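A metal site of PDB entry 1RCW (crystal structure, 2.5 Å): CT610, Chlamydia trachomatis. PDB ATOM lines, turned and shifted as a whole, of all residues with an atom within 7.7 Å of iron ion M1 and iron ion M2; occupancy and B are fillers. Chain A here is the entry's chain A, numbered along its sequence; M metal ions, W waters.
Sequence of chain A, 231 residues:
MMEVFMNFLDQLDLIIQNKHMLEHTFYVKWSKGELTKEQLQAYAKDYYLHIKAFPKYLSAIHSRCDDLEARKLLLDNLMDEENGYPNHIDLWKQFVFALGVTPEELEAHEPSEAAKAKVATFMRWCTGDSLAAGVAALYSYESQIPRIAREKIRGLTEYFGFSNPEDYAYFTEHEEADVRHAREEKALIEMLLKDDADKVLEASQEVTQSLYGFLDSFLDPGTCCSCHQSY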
ATOM      1  N   ILE A  51     -22.346  12.595  14.000  1.00  0.00           N
ATOM      2  CA  ILE A  51     -22.150  11.501  13.091  1.00  0.00           C
ATOM      3  C   ILE A  51     -22.122  12.016  11.637  1.00  0.00           C
ATOM      4  O   ILE A  51     -21.300  11.609  10.873  1.00  0.00           O
ATOM      5  CB  ILE A  51     -23.285  10.467  13.300  1.00  0.00           C
ATOM      6  CG1 ILE A  51     -23.163   9.798  14.684  1.00  0.00           C
ATOM      7  CG2 ILE A  51     -23.282   9.357  12.243  1.00  0.00           C
ATOM      8  CD1 ILE A  51     -21.886   9.049  14.943  1.00  0.00           C
ATOM      9  N   PHE A  54     -18.988  14.154  11.014  1.00  0.00           N
ATOM     10  CA  PHE A  54     -17.656  13.598  11.139  1.00  0.00           C
ATOM     11  C   PHE A  54     -16.862  13.630   9.828  1.00  0.00           C
ATOM     12  O   PHE A  54     -15.744  14.113   9.842  1.00  0.00           O
ATOM     13  CB  PHE A  54     -17.667  12.196  11.723  1.00  0.00           C
ATOM     14  CG  PHE A  54     -16.419  11.886  12.399  1.00  0.00           C
ATOM     15  CD1 PHE A  54     -16.236  12.234  13.713  1.00  0.00           C
ATOM     16  CD2 PHE A  54     -15.368  11.340  11.709  1.00  0.00           C
ATOM     17  CE1 PHE A  54     -15.030  11.980  14.346  1.00  0.00           C
ATOM     18  CE2 PHE A  54     -14.175  11.096  12.345  1.00  0.00           C
ATOM     19  CZ  PHE A  54     -13.999  11.427  13.646  1.00  0.00           C
ATOM     20  N   LEU A  58     -12.895  15.540   8.689  1.00  0.00           N
ATOM     21  CA  LEU A  58     -11.749  14.972   7.943  1.00  0.00           C
ATOM     22  C   LEU A  58     -11.408  15.712   6.646  1.00  0.00           C
ATOM     23  O   LEU A  58     -10.250  15.989   6.367  1.00  0.00           O
ATOM     24  CB  LEU A  58     -12.017  13.482   7.658  1.00  0.00           C
ATOM     25  CG  LEU A  58     -11.988  12.576   8.898  1.00  0.00           C
ATOM     26  CD1 LEU A  58     -12.675  11.259   8.678  1.00  0.00           C
ATOM     27  CD2 LEU A  58     -10.567  12.302   9.287  1.00  0.00           C
ATOM     28  N   ASN A  77      -9.239   7.329   6.028  1.00  0.00           N
ATOM     29  CA  ASN A  77     -10.284   7.439   7.070  1.00  0.00           C
ATOM     30  C   ASN A  77     -11.648   7.887   6.481  1.00  0.00           C
ATOM     31  O   ASN A  77     -12.708   7.356   6.798  1.00  0.00           O
ATOM     32  CB  ASN A  77      -9.858   8.399   8.175  1.00  0.00           C
ATOM     33  CG  ASN A  77      -8.851   7.769   9.196  1.00  0.00           C
ATOM     34  OD1 ASN A  77      -8.105   6.792   8.894  1.00  0.00           O
ATOM     35  ND2 ASN A  77      -8.819   8.342  10.401  1.00  0.00           N
ATOM     36  N   ASP A  80     -13.503   5.047   4.734  1.00  0.00           N
ATOM     37  CA  ASP A  80     -14.073   4.158   5.718  1.00  0.00           C
ATOM     38  C   ASP A  80     -15.347   4.746   6.308  1.00  0.00           C
ATOM     39  O   ASP A  80     -16.284   4.013   6.538  1.00  0.00           O
ATOM     40  CB  ASP A  80     -13.121   3.914   6.905  1.00  0.00           C
ATOM     41  CG  ASP A  80     -11.935   3.002   6.582  1.00  0.00           C
ATOM     42  OD1 ASP A  80     -11.931   2.303   5.530  1.00  0.00           O
ATOM     43  OD2 ASP A  80     -10.933   2.925   7.372  1.00  0.00           O
ATOM     44  N   GLU A  81     -15.390   6.052   6.564  1.00  0.00           N
ATOM     45  CA  GLU A  81     -16.589   6.633   7.208  1.00  0.00           C
ATOM     46  C   GLU A  81     -17.755   6.709   6.261  1.00  0.00           C
ATOM     47  O   GLU A  81     -18.888   6.494   6.637  1.00  0.00           O
ATOM     48  CB  GLU A  81     -16.352   8.063   7.733  1.00  0.00           C
ATOM     49  CG  GLU A  81     -15.156   8.247   8.664  1.00  0.00           C
ATOM     50  CD  GLU A  81     -15.294   7.538  10.002  1.00  0.00           C
ATOM     51  OE1 GLU A  81     -14.259   7.289  10.675  1.00  0.00           O
ATOM     52  OE2 GLU A  81     -16.455   7.243  10.364  1.00  0.00           O
ATOM     53  N   GLU A  82     -17.487   7.049   5.019  1.00  0.00           N
ATOM     54  CA  GLU A  82     -18.550   7.594   4.154  1.00  0.00           C
ATOM     55  C   GLU A  82     -18.776   6.850   2.824  1.00  0.00           C
ATOM     56  O   GLU A  82     -19.858   6.963   2.267  1.00  0.00           O
ATOM     57  CB  GLU A  82     -18.341   9.109   3.930  1.00  0.00           C
ATOM     58  CG  GLU A  82     -19.610   9.874   3.654  1.00  0.00           C
ATOM     59  CD  GLU A  82     -19.411  11.355   3.343  1.00  0.00           C
ATOM     60  OE1 GLU A  82     -18.336  11.764   2.829  1.00  0.00           O
ATOM     61  OE2 GLU A  82     -20.352  12.114   3.564  1.00  0.00           O
ATOM     62  N   ASN A  87     -22.727   2.924   4.923  1.00  0.00           N
ATOM     63  CA  ASN A  87     -21.603   3.637   5.537  1.00  0.00           C
ATOM     64  C   ASN A  87     -21.886   3.891   7.018  1.00  0.00           C
ATOM     65  O   ASN A  87     -22.940   3.490   7.543  1.00  0.00           O
ATOM     66  CB  ASN A  87     -21.289   4.937   4.796  1.00  0.00           C
ATOM     67  CG  ASN A  87     -22.369   5.979   4.958  1.00  0.00           C
ATOM     68  OD1 ASN A  87     -23.211   5.897   5.854  1.00  0.00           O
ATOM     69  ND2 ASN A  87     -22.376   6.944   4.075  1.00  0.00           N
ATOM     70  N   HIS A  88     -20.970   4.579   7.698  1.00  0.00           N
ATOM     71  CA  HIS A  88     -21.117   4.732   9.142  1.00  0.00           C
ATOM     72  C   HIS A  88     -22.389   5.507   9.490  1.00  0.00           C
ATOM     73  O   HIS A  88     -23.076   5.153  10.419  1.00  0.00           O
ATOM     74  CB  HIS A  88     -19.811   5.289   9.786  1.00  0.00           C
ATOM     75  CG  HIS A  88     -18.693   4.282   9.741  1.00  0.00           C
ATOM     76  ND1 HIS A  88     -17.501   4.443  10.396  1.00  0.00           N
ATOM     77  CD2 HIS A  88     -18.613   3.090   9.086  1.00  0.00           C
ATOM     78  CE1 HIS A  88     -16.714   3.401  10.132  1.00  0.00           C
ATOM     79  NE2 HIS A  88     -17.372   2.556   9.364  1.00  0.00           N
ATOM     80  N   ILE A  89     -22.753   6.512   8.696  1.00  0.00           N
ATOM     81  CA  ILE A  89     -23.999   7.199   8.933  1.00  0.00           C
ATOM     82  C   ILE A  89     -25.157   6.224   8.811  1.00  0.00           C
ATOM     83  O   ILE A  89     -25.978   6.107   9.718  1.00  0.00           O
ATOM     84  CB  ILE A  89     -24.167   8.420   8.004  1.00  0.00           C
ATOM     85  CG1 ILE A  89     -23.145   9.507   8.353  1.00  0.00           C
ATOM     86  CG2 ILE A  89     -25.537   9.045   8.140  1.00  0.00           C
ATOM     87  CD1 ILE A  89     -22.765  10.342   7.150  1.00  0.00           C
ATOM     88  N   LEU A  91     -25.187   3.111   9.269  1.00  0.00           N
ATOM     89  CA  LEU A  91     -25.188   2.163  10.352  1.00  0.00           C
ATOM     90  C   LEU A  91     -25.730   2.820  11.600  1.00  0.00           C
ATOM     91  O   LEU A  91     -26.476   2.188  12.380  1.00  0.00           O
ATOM     92  CB  LEU A  91     -23.812   1.588  10.629  1.00  0.00           C
ATOM     93  CG  LEU A  91     -23.198   0.731   9.532  1.00  0.00           C
ATOM     94  CD1 LEU A  91     -21.761   0.334   9.880  1.00  0.00           C
ATOM     95  CD2 LEU A  91     -23.998  -0.496   9.293  1.00  0.00           C
ATOM     96  N   TYR A 141     -11.453  11.746  20.325  1.00  0.00           N
ATOM     97  CA  TYR A 141     -12.750  11.053  20.331  1.00  0.00           C
ATOM     98  C   TYR A 141     -12.562   9.618  19.806  1.00  0.00           C
ATOM     99  O   TYR A 141     -12.823   8.644  20.488  1.00  0.00           O
ATOM    100  CB  TYR A 141     -13.748  11.846  19.455  1.00  0.00           C
ATOM    101  CG  TYR A 141     -15.106  11.169  19.224  1.00  0.00           C
ATOM    102  CD1 TYR A 141     -16.091  11.221  20.190  1.00  0.00           C
ATOM    103  CD2 TYR A 141     -15.386  10.504  18.031  1.00  0.00           C
ATOM    104  CE1 TYR A 141     -17.329  10.603  19.976  1.00  0.00           C
ATOM    105  CE2 TYR A 141     -16.645   9.880  17.807  1.00  0.00           C
ATOM    106  CZ  TYR A 141     -17.588   9.950  18.780  1.00  0.00           C
ATOM    107  OH  TYR A 141     -18.807   9.364  18.601  1.00  0.00           O
ATOM    108  N   GLU A 142     -12.049   9.484  18.599  1.00  0.00           N
ATOM    109  CA  GLU A 142     -11.887   8.175  18.011  1.00  0.00           C
ATOM    110  C   GLU A 142     -11.066   7.239  18.899  1.00  0.00           C
ATOM    111  O   GLU A 142     -11.390   6.065  18.988  1.00  0.00           O
ATOM    112  CB  GLU A 142     -11.370   8.233  16.549  1.00  0.00           C
ATOM    113  CG  GLU A 142     -12.536   8.417  15.595  1.00  0.00           C
ATOM    114  CD  GLU A 142     -12.203   8.405  14.117  1.00  0.00           C
ATOM    115  OE1 GLU A 142     -12.855   7.638  13.367  1.00  0.00           O
ATOM    116  OE2 GLU A 142     -11.358   9.197  13.709  1.00  0.00           O
ATOM    117  N   ILE A 145     -13.391   5.254  21.123  1.00  0.00           N
ATOM    118  CA  ILE A 145     -14.534   4.477  20.635  1.00  0.00           C
ATOM    119  C   ILE A 145     -14.375   2.933  20.677  1.00  0.00           C
ATOM    120  O   ILE A 145     -15.326   2.242  21.063  1.00  0.00           O
ATOM    121  CB  ILE A 145     -14.961   4.993  19.254  1.00  0.00           C
ATOM    122  CG1 ILE A 145     -15.558   6.415  19.370  1.00  0.00           C
ATOM    123  CG2 ILE A 145     -15.964   4.066  18.623  1.00  0.00           C
ATOM    124  CD1 ILE A 145     -16.996   6.478  19.978  1.00  0.00           C
ATOM    125  N   TYR A 170     -23.264  -0.795  13.936  1.00  0.00           N
ATOM    126  CA  TYR A 170     -22.410   0.395  14.037  1.00  0.00           C
ATOM    127  C   TYR A 170     -21.287   0.126  14.991  1.00  0.00           C
ATOM    128  O   TYR A 170     -20.158   0.521  14.736  1.00  0.00           O
ATOM    129  CB  TYR A 170     -23.170   1.631  14.540  1.00  0.00           C
ATOM    130  CG  TYR A 170     -22.309   2.880  14.654  1.00  0.00           C
ATOM    131  CD1 TYR A 170     -22.103   3.731  13.554  1.00  0.00           C
ATOM    132  CD2 TYR A 170     -21.676   3.209  15.852  1.00  0.00           C
ATOM    133  CE1 TYR A 170     -21.270   4.895  13.668  1.00  0.00           C
ATOM    134  CE2 TYR A 170     -20.858   4.359  15.976  1.00  0.00           C
ATOM    135  CZ  TYR A 170     -20.659   5.189  14.905  1.00  0.00           C
ATOM    136  OH  TYR A 170     -19.858   6.302  15.076  1.00  0.00           O
ATOM    137  N   GLU A 173     -18.874  -2.546  13.984  1.00  0.00           N
ATOM    138  CA  GLU A 173     -17.953  -1.930  13.041  1.00  0.00           C
ATOM    139  C   GLU A 173     -16.840  -1.167  13.754  1.00  0.00           C
ATOM    140  O   GLU A 173     -15.639  -1.371  13.433  1.00  0.00           O
ATOM    141  CB  GLU A 173     -18.693  -0.960  12.086  1.00  0.00           C
ATOM    142  CG  GLU A 173     -18.665  -1.379  10.614  1.00  0.00           C
ATOM    143  CD  GLU A 173     -17.261  -1.751  10.169  1.00  0.00           C
ATOM    144  OE1 GLU A 173     -16.439  -0.823   9.986  1.00  0.00           O
ATOM    145  OE2 GLU A 173     -16.996  -2.976  10.025  1.00  0.00           O
ATOM    146  N   HIS A 174     -17.244  -0.338  14.723  1.00  0.00           N
ATOM    147  CA  HIS A 174     -16.340   0.585  15.363  1.00  0.00           C
ATOM    148  C   HIS A 174     -15.361  -0.046  16.383  1.00  0.00           C
ATOM    149  O   HIS A 174     -14.242   0.470  16.550  1.00  0.00           O
ATOM    150  CB  HIS A 174     -17.124   1.753  15.939  1.00  0.00           C
ATOM    151  CG  HIS A 174     -17.557   2.705  14.893  1.00  0.00           C
ATOM    152  ND1 HIS A 174     -18.505   2.368  13.956  1.00  0.00           N
ATOM    153  CD2 HIS A 174     -17.081   3.909  14.535  1.00  0.00           C
ATOM    154  CE1 HIS A 174     -18.647   3.364  13.101  1.00  0.00           C
ATOM    155  NE2 HIS A 174     -17.788   4.316  13.436  1.00  0.00           N
ATOM    156  N   ALA A 177     -12.807  -0.802  13.438  1.00  0.00           N
ATOM    157  CA  ALA A 177     -12.459   0.294  12.524  1.00  0.00           C
ATOM    158  C   ALA A 177     -11.656   1.378  13.215  1.00  0.00           C
ATOM    159  O   ALA A 177     -10.617   1.826  12.706  1.00  0.00           O
ATOM    160  CB  ALA A 177     -13.716   0.895  11.924  1.00  0.00           C
ATOM    161  N   ASP A 178     -12.104   1.773  14.400  1.00  0.00           N
ATOM    162  CA  ASP A 178     -11.462   2.883  15.042  1.00  0.00           C
ATOM    163  C   ASP A 178     -10.128   2.529  15.661  1.00  0.00           C
ATOM    164  O   ASP A 178      -9.369   3.444  16.009  1.00  0.00           O
ATOM    165  CB  ASP A 178     -12.398   3.583  16.028  1.00  0.00           C
ATOM    166  CG  ASP A 178     -13.431   4.439  15.337  1.00  0.00           C
ATOM    167  OD1 ASP A 178     -13.533   4.356  14.116  1.00  0.00           O
ATOM    168  OD2 ASP A 178     -14.210   5.210  15.934  1.00  0.00           O
ATOM    169  N   VAL A 179      -9.809   1.238  15.773  1.00  0.00           N
ATOM    170  CA  VAL A 179      -8.447   0.861  16.214  1.00  0.00           C
ATOM    171  C   VAL A 179      -7.498   1.379  15.127  1.00  0.00           C
ATOM    172  O   VAL A 179      -6.504   2.050  15.423  1.00  0.00           O
ATOM    173  CB  VAL A 179      -8.238  -0.699  16.432  1.00  0.00           C
ATOM    174  CG1 VAL A 179      -6.812  -0.993  16.694  1.00  0.00           C
ATOM    175  CG2 VAL A 179      -9.027  -1.185  17.589  1.00  0.00           C
ATOM    176  N   ARG A 180      -7.847   1.071  13.873  1.00  0.00           N
ATOM    177  CA  ARG A 180      -7.094   1.555  12.721  1.00  0.00           C
ATOM    178  C   ARG A 180      -7.055   3.071  12.707  1.00  0.00           C
ATOM    179  O   ARG A 180      -5.994   3.672  12.557  1.00  0.00           O
ATOM    180  CB  ARG A 180      -7.731   1.062  11.415  1.00  0.00           C
ATOM    181  CG  ARG A 180      -6.981   1.424  10.155  1.00  0.00           C
ATOM    182  CD  ARG A 180      -7.499   0.702   8.873  1.00  0.00           C
ATOM    183  NE  ARG A 180      -8.949   0.769   8.690  1.00  0.00           N
ATOM    184  CZ  ARG A 180      -9.835  -0.170   9.061  1.00  0.00           C
ATOM    185  NH1 ARG A 180      -9.450  -1.290   9.667  1.00  0.00           N
ATOM    186  NH2 ARG A 180     -11.136   0.016   8.842  1.00  0.00           N
ATOM    187  N   HIS A 181      -8.207   3.702  12.862  1.00  0.00           N
ATOM    188  CA  HIS A 181      -8.220   5.155  12.720  1.00  0.00           C
ATOM    189  C   HIS A 181      -7.426   5.850  13.809  1.00  0.00           C
ATOM    190  O   HIS A 181      -6.833   6.902  13.532  1.00  0.00           O
ATOM    191  CB  HIS A 181      -9.647   5.709  12.688  1.00  0.00           C
ATOM    192  CG  HIS A 181     -10.439   5.215  11.532  1.00  0.00           C
ATOM    193  ND1 HIS A 181     -11.801   5.366  11.448  1.00  0.00           N
ATOM    194  CD2 HIS A 181     -10.050   4.552  10.418  1.00  0.00           C
ATOM    195  CE1 HIS A 181     -12.232   4.813  10.324  1.00  0.00           C
ATOM    196  NE2 HIS A 181     -11.190   4.303   9.683  1.00  0.00           N
ATOM    197  N   ALA A 182      -7.410   5.292  15.018  1.00  0.00           N
ATOM    198  CA  ALA A 182      -6.651   5.905  16.100  1.00  0.00           C
ATOM    199  C   ALA A 182      -5.195   5.828  15.787  1.00  0.00           C
ATOM    200  O   ALA A 182      -4.477   6.785  15.916  1.00  0.00           O
ATOM    201  CB  ALA A 182      -6.958   5.239  17.431  1.00  0.00           C
ATOM    202  N   GLU A 185      -4.392   8.333  13.037  1.00  0.00           N
ATOM    203  CA  GLU A 185      -4.423   9.692  13.543  1.00  0.00           C
ATOM    204  C   GLU A 185      -3.210  10.044  14.382  1.00  0.00           C
ATOM    205  O   GLU A 185      -2.694  11.178  14.265  1.00  0.00           O
ATOM    206  CB  GLU A 185      -5.690   9.952  14.291  1.00  0.00           C
ATOM    207  CG  GLU A 185      -6.871   9.909  13.349  1.00  0.00           C
ATOM    208  CD  GLU A 185      -8.200   9.756  14.037  1.00  0.00           C
ATOM    209  OE1 GLU A 185      -9.161   9.862  13.288  1.00  0.00           O
ATOM    210  OE2 GLU A 185      -8.255   9.557  15.275  1.00  0.00           O
HETATM  211 FE    FE M   1     -13.737   6.184  12.704  1.00  0.00          FE
HETATM  212 FE    FE M   2     -16.903   5.855  12.013  1.00  0.00          FE
HETATM  213  O   HOH W   1     -18.674   7.180  12.498  1.00  0.00           O
HETATM  214  O   HOH W   2     -15.978   7.770  14.179  1.00  0.00           O
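Of the 24 residues printed, 3 come within 4 Å of iron ion M2.
O of Tyr 170 lies within hydrogen-bond range of ND1 of His 174 (2.6 Å).
NE2 of His 88 is in hydrogen-bond range of O of Asp 80, at 3.4 Å.
NE2 of His 181 is in hydrogen-bond range of OD2 of Asp 80, at 2.7 Å.
Iron ion M2 is bound by the side-chain carboxylate of Glu 81 (2.2 Å), a ring nitrogen (ND1) of His 88 (2.2 Å), water W1 (2.3 Å) and a ring nitrogen (NE2) of His 174 (2.3 Å).
Iron ion M1 is bound by the side-chain carboxylate (OE1) of Glu 142 (1.8 Å), the side-chain carboxylate (OD1) of Asp 178 (2.3 Å), the side-chain carboxylate (OE1) of Glu 81 (2.4 Å) and a ring nitrogen (ND1) of His 181 (2.4 Å).
Iron ion M1 has four donor atoms within binding distance.
Within 4 Å of iron ion M1: Glu 81, Glu 142, Asp 178 and His 181.
The nearest printed residue that does not touch iron ion M1 is His 174 (4.4 Å).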
